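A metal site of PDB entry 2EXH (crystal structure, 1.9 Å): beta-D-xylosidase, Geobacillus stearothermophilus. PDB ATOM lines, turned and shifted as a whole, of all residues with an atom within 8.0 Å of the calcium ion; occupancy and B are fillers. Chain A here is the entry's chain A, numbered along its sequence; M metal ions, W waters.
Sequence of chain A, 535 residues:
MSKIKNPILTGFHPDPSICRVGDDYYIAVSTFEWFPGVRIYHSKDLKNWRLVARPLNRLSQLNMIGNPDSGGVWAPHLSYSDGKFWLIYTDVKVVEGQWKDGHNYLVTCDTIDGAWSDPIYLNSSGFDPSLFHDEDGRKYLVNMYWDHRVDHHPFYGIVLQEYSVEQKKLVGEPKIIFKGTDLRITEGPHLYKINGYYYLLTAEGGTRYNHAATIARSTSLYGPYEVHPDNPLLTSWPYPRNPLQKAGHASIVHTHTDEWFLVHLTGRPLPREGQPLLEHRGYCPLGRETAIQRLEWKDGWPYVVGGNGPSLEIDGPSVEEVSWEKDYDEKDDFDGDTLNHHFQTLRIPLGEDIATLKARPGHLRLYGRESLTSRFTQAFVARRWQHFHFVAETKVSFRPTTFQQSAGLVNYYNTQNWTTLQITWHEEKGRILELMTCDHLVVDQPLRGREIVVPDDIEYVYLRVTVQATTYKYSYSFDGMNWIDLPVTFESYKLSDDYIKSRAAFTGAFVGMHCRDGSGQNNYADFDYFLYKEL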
ATOM      1  N   LYS A 331      18.343 -12.678 -10.698  1.00  0.00           N
ATOM      2  CA  LYS A 331      17.254 -12.208  -9.837  1.00  0.00           C
ATOM      3  C   LYS A 331      15.928 -12.337 -10.594  1.00  0.00           C
ATOM      4  O   LYS A 331      15.537 -11.465 -11.365  1.00  0.00           O
ATOM      5  CB  LYS A 331      17.512 -10.770  -9.374  1.00  0.00           C
ATOM      6  CG  LYS A 331      16.485 -10.205  -8.389  1.00  0.00           C
ATOM      7  CD  LYS A 331      17.009  -8.929  -7.733  1.00  0.00           C
ATOM      8  CE  LYS A 331      15.887  -8.125  -7.095  1.00  0.00           C
ATOM      9  NZ  LYS A 331      16.380  -6.853  -6.470  1.00  0.00           N
ATOM     10  N   ASP A 332      15.261 -13.466 -10.374  1.00  0.00           N
ATOM     11  CA  ASP A 332      13.983 -13.725 -11.011  1.00  0.00           C
ATOM     12  C   ASP A 332      12.924 -12.911 -10.262  1.00  0.00           C
ATOM     13  O   ASP A 332      12.583 -13.237  -9.119  1.00  0.00           O
ATOM     14  CB  ASP A 332      13.665 -15.221 -10.973  1.00  0.00           C
ATOM     15  CG  ASP A 332      12.371 -15.582 -11.671  1.00  0.00           C
ATOM     16  OD1 ASP A 332      11.526 -14.687 -11.904  1.00  0.00           O
ATOM     17  OD2 ASP A 332      12.179 -16.779 -11.979  1.00  0.00           O
ATOM     18  N   ASP A 333      12.445 -11.845 -10.901  1.00  0.00           N
ATOM     19  CA  ASP A 333      11.405 -11.000 -10.280  1.00  0.00           C
ATOM     20  C   ASP A 333       9.969 -11.466 -10.489  1.00  0.00           C
ATOM     21  O   ASP A 333       9.028 -10.755 -10.125  1.00  0.00           O
ATOM     22  CB  ASP A 333      11.552  -9.529 -10.663  1.00  0.00           C
ATOM     23  CG  ASP A 333      11.849  -8.654  -9.459  1.00  0.00           C
ATOM     24  OD1 ASP A 333      10.878  -8.148  -8.828  1.00  0.00           O
ATOM     25  OD2 ASP A 333      13.041  -8.499  -9.109  1.00  0.00           O
ATOM     26  N   PHE A 334       9.806 -12.682 -11.027  1.00  0.00           N
ATOM     27  CA  PHE A 334       8.477 -13.282 -11.257  1.00  0.00           C
ATOM     28  C   PHE A 334       7.608 -12.425 -12.188  1.00  0.00           C
ATOM     29  O   PHE A 334       6.471 -12.071 -11.856  1.00  0.00           O
ATOM     30  CB  PHE A 334       7.754 -13.586  -9.923  1.00  0.00           C
ATOM     31  CG  PHE A 334       8.487 -14.564  -9.041  1.00  0.00           C
ATOM     32  CD1 PHE A 334       8.881 -15.809  -9.531  1.00  0.00           C
ATOM     33  CD2 PHE A 334       8.762 -14.259  -7.709  1.00  0.00           C
ATOM     34  CE1 PHE A 334       9.544 -16.725  -8.715  1.00  0.00           C
ATOM     35  CE2 PHE A 334       9.424 -15.173  -6.883  1.00  0.00           C
ATOM     36  CZ  PHE A 334       9.824 -16.399  -7.387  1.00  0.00           C
ATOM     37  N   ASP A 335       8.166 -12.099 -13.357  1.00  0.00           N
ATOM     38  CA  ASP A 335       7.528 -11.222 -14.339  1.00  0.00           C
ATOM     39  C   ASP A 335       6.691 -11.982 -15.353  1.00  0.00           C
ATOM     40  O   ASP A 335       5.678 -11.461 -15.839  1.00  0.00           O
ATOM     41  CB  ASP A 335       8.575 -10.426 -15.115  1.00  0.00           C
ATOM     42  CG  ASP A 335       9.356  -9.467 -14.235  1.00  0.00           C
ATOM     43  OD1 ASP A 335       8.747  -8.812 -13.362  1.00  0.00           O
ATOM     44  OD2 ASP A 335      10.587  -9.376 -14.433  1.00  0.00           O
ATOM     45  N   ARG A 360      -1.071 -11.502  -7.074  1.00  0.00           N
ATOM     46  CA  ARG A 360      -0.361 -10.238  -6.810  1.00  0.00           C
ATOM     47  C   ARG A 360       0.713 -10.053  -7.858  1.00  0.00           C
ATOM     48  O   ARG A 360       1.695 -10.795  -7.878  1.00  0.00           O
ATOM     49  CB  ARG A 360       0.263 -10.226  -5.411  1.00  0.00           C
ATOM     50  CG  ARG A 360       0.798  -8.831  -5.004  1.00  0.00           C
ATOM     51  CD  ARG A 360       1.353  -8.870  -3.606  1.00  0.00           C
ATOM     52  NE  ARG A 360       1.929  -7.589  -3.195  1.00  0.00           N
ATOM     53  CZ  ARG A 360       2.568  -7.394  -2.047  1.00  0.00           C
ATOM     54  NH1 ARG A 360       2.734  -8.384  -1.195  1.00  0.00           N
ATOM     55  NH2 ARG A 360       3.059  -6.196  -1.764  1.00  0.00           N
ATOM     56  N   PRO A 361       0.550  -9.036  -8.736  1.00  0.00           N
ATOM     57  CA  PRO A 361       1.464  -8.881  -9.872  1.00  0.00           C
ATOM     58  C   PRO A 361       2.938  -8.808  -9.469  1.00  0.00           C
ATOM     59  O   PRO A 361       3.283  -8.180  -8.448  1.00  0.00           O
ATOM     60  CB  PRO A 361       0.999  -7.555 -10.504  1.00  0.00           C
ATOM     61  CG  PRO A 361      -0.430  -7.419 -10.081  1.00  0.00           C
ATOM     62  CD  PRO A 361      -0.465  -7.969  -8.692  1.00  0.00           C
ATOM     63  N   GLY A 362       3.778  -9.467 -10.255  1.00  0.00           N
ATOM     64  CA  GLY A 362       5.212  -9.531  -9.997  1.00  0.00           C
ATOM     65  C   GLY A 362       5.587 -10.281  -8.731  1.00  0.00           C
ATOM     66  O   GLY A 362       6.692 -10.127  -8.219  1.00  0.00           O
ATOM     67  N   HIS A 363       4.659 -11.090  -8.215  1.00  0.00           N
ATOM     68  CA  HIS A 363       4.913 -11.901  -7.031  1.00  0.00           C
ATOM     69  C   HIS A 363       4.453 -13.324  -7.267  1.00  0.00           C
ATOM     70  O   HIS A 363       3.415 -13.550  -7.905  1.00  0.00           O
ATOM     71  CB  HIS A 363       4.169 -11.356  -5.811  1.00  0.00           C
ATOM     72  CG  HIS A 363       4.637 -10.009  -5.345  1.00  0.00           C
ATOM     73  ND1 HIS A 363       4.370  -8.854  -6.039  1.00  0.00           N
ATOM     74  CD2 HIS A 363       5.332  -9.641  -4.252  1.00  0.00           C
ATOM     75  CE1 HIS A 363       4.896  -7.823  -5.393  1.00  0.00           C
ATOM     76  NE2 HIS A 363       5.488  -8.278  -4.306  1.00  0.00           N
ATOM     77  N   LEU A 364       5.219 -14.279  -6.767  1.00  0.00           N
ATOM     78  CA  LEU A 364       4.721 -15.629  -6.611  1.00  0.00           C
ATOM     79  C   LEU A 364       3.981 -15.673  -5.279  1.00  0.00           C
ATOM     80  O   LEU A 364       4.587 -15.400  -4.220  1.00  0.00           O
ATOM     81  CB  LEU A 364       5.875 -16.626  -6.605  1.00  0.00           C
ATOM     82  CG  LEU A 364       5.536 -18.085  -6.269  1.00  0.00           C
ATOM     83  CD1 LEU A 364       4.545 -18.691  -7.257  1.00  0.00           C
ATOM     84  CD2 LEU A 364       6.821 -18.867  -6.213  1.00  0.00           C
ATOM     85  N   LYS A 395      12.513 -12.367  -1.057  1.00  0.00           N
ATOM     86  CA  LYS A 395      11.919 -11.241  -0.373  1.00  0.00           C
ATOM     87  C   LYS A 395      10.428 -11.541  -0.281  1.00  0.00           C
ATOM     88  O   LYS A 395       9.763 -11.780  -1.307  1.00  0.00           O
ATOM     89  CB  LYS A 395      12.195  -9.963  -1.184  1.00  0.00           C
ATOM     90  CG  LYS A 395      11.423  -8.708  -0.765  1.00  0.00           C
ATOM     91  CD  LYS A 395      11.560  -7.641  -1.841  1.00  0.00           C
ATOM     92  CE  LYS A 395      10.663  -6.443  -1.576  1.00  0.00           C
ATOM     93  NZ  LYS A 395      10.741  -5.432  -2.693  1.00  0.00           N
ATOM     94  N   TYR A 460       8.173  -6.407   4.003  1.00  0.00           N
ATOM     95  CA  TYR A 460       8.933  -7.516   3.441  1.00  0.00           C
ATOM     96  C   TYR A 460      10.083  -7.956   4.333  1.00  0.00           C
ATOM     97  O   TYR A 460      10.848  -7.141   4.854  1.00  0.00           O
ATOM     98  CB  TYR A 460       9.488  -7.129   2.065  1.00  0.00           C
ATOM     99  CG  TYR A 460       8.471  -6.984   0.962  1.00  0.00           C
ATOM    100  CD1 TYR A 460       7.949  -8.109   0.316  1.00  0.00           C
ATOM    101  CD2 TYR A 460       8.053  -5.729   0.531  1.00  0.00           C
ATOM    102  CE1 TYR A 460       7.033  -7.985  -0.719  1.00  0.00           C
ATOM    103  CE2 TYR A 460       7.131  -5.587  -0.509  1.00  0.00           C
ATOM    104  CZ  TYR A 460       6.624  -6.724  -1.132  1.00  0.00           C
ATOM    105  OH  TYR A 460       5.707  -6.598  -2.157  1.00  0.00           O
ATOM    106  N   PHE A 527       5.999 -13.673  -2.525  1.00  0.00           N
ATOM    107  CA  PHE A 527       7.434 -13.614  -2.784  1.00  0.00           C
ATOM    108  C   PHE A 527       7.719 -12.687  -3.960  1.00  0.00           C
ATOM    109  O   PHE A 527       7.323 -12.980  -5.083  1.00  0.00           O
ATOM    110  CB  PHE A 527       7.979 -15.013  -3.096  1.00  0.00           C
ATOM    111  CG  PHE A 527       7.871 -15.985  -1.957  1.00  0.00           C
ATOM    112  CD1 PHE A 527       8.916 -16.143  -1.045  1.00  0.00           C
ATOM    113  CD2 PHE A 527       6.712 -16.751  -1.792  1.00  0.00           C
ATOM    114  CE1 PHE A 527       8.815 -17.036   0.006  1.00  0.00           C
ATOM    115  CE2 PHE A 527       6.598 -17.631  -0.713  1.00  0.00           C
ATOM    116  CZ  PHE A 527       7.661 -17.778   0.177  1.00  0.00           C
ATOM    117  N   ASP A 528       8.420 -11.586  -3.704  1.00  0.00           N
ATOM    118  CA  ASP A 528       8.647 -10.582  -4.745  1.00  0.00           C
ATOM    119  C   ASP A 528       9.670 -11.027  -5.806  1.00  0.00           C
ATOM    120  O   ASP A 528       9.523 -10.738  -6.992  1.00  0.00           O
ATOM    121  CB  ASP A 528       9.032  -9.254  -4.113  1.00  0.00           C
ATOM    122  CG  ASP A 528       9.255  -8.152  -5.133  1.00  0.00           C
ATOM    123  OD1 ASP A 528      10.046  -7.227  -4.828  1.00  0.00           O
ATOM    124  OD2 ASP A 528       8.683  -8.207  -6.257  1.00  0.00           O
ATOM    125  N   TYR A 529      10.716 -11.718  -5.365  1.00  0.00           N
ATOM    126  CA  TYR A 529      11.746 -12.246  -6.277  1.00  0.00           C
ATOM    127  C   TYR A 529      12.413 -13.485  -5.690  1.00  0.00           C
ATOM    128  O   TYR A 529      12.279 -13.766  -4.501  1.00  0.00           O
ATOM    129  CB  TYR A 529      12.794 -11.166  -6.611  1.00  0.00           C
ATOM    130  CG  TYR A 529      13.669 -10.684  -5.457  1.00  0.00           C
ATOM    131  CD1 TYR A 529      14.755 -11.447  -5.011  1.00  0.00           C
ATOM    132  CD2 TYR A 529      13.410  -9.466  -4.826  1.00  0.00           C
ATOM    133  CE1 TYR A 529      15.556 -11.015  -3.950  1.00  0.00           C
ATOM    134  CE2 TYR A 529      14.207  -9.015  -3.769  1.00  0.00           C
ATOM    135  CZ  TYR A 529      15.267  -9.800  -3.339  1.00  0.00           C
ATOM    136  OH  TYR A 529      16.054  -9.356  -2.302  1.00  0.00           O
ATOM    137  N   PHE A 530      13.092 -14.245  -6.550  1.00  0.00           N
ATOM    138  CA  PHE A 530      13.960 -15.322  -6.105  1.00  0.00           C
ATOM    139  C   PHE A 530      15.274 -15.216  -6.835  1.00  0.00           C
ATOM    140  O   PHE A 530      15.321 -15.202  -8.073  1.00  0.00           O
ATOM    141  CB  PHE A 530      13.336 -16.711  -6.321  1.00  0.00           C
ATOM    142  CG  PHE A 530      14.170 -17.835  -5.754  1.00  0.00           C
ATOM    143  CD1 PHE A 530      14.033 -18.203  -4.424  1.00  0.00           C
ATOM    144  CD2 PHE A 530      15.095 -18.503  -6.547  1.00  0.00           C
ATOM    145  CE1 PHE A 530      14.799 -19.235  -3.889  1.00  0.00           C
ATOM    146  CE2 PHE A 530      15.872 -19.535  -6.021  1.00  0.00           C
ATOM    147  CZ  PHE A 530      15.722 -19.894  -4.683  1.00  0.00           C
HETATM  148 CA    CA M   1       8.612  -9.041  -8.445  1.00  0.00          CA
HETATM  149  O   HOH W   1       8.389  -8.142 -10.750  1.00  0.00           O
HETATM  150  O   HOH W   2       7.386  -6.884  -8.580  1.00  0.00           O
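The calcium ion is bound by O of Gly 362, at 2.2 Å. The side-chain carboxylate (OD2) of Asp 528 binds the calcium ion. O of Asp 528 binds the calcium ion (2.4 Å). O of Asp 333 binds the calcium ion (2.4 Å). The side-chain carboxylate (OD1) of Asp 333 is bound to the calcium ion (2.5 Å). Water W1 is bound to the calcium ion, at 2.5 Å. The calcium ion is bound by water W2, 2.5 Å away. The calcium ion has seven donor atoms within binding distance.
Of the 16 residues printed, 3 come within 4 Å of the calcium ion.
NZ of Lys 395 lies within salt-bridge range of OD1 of Asp 528.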
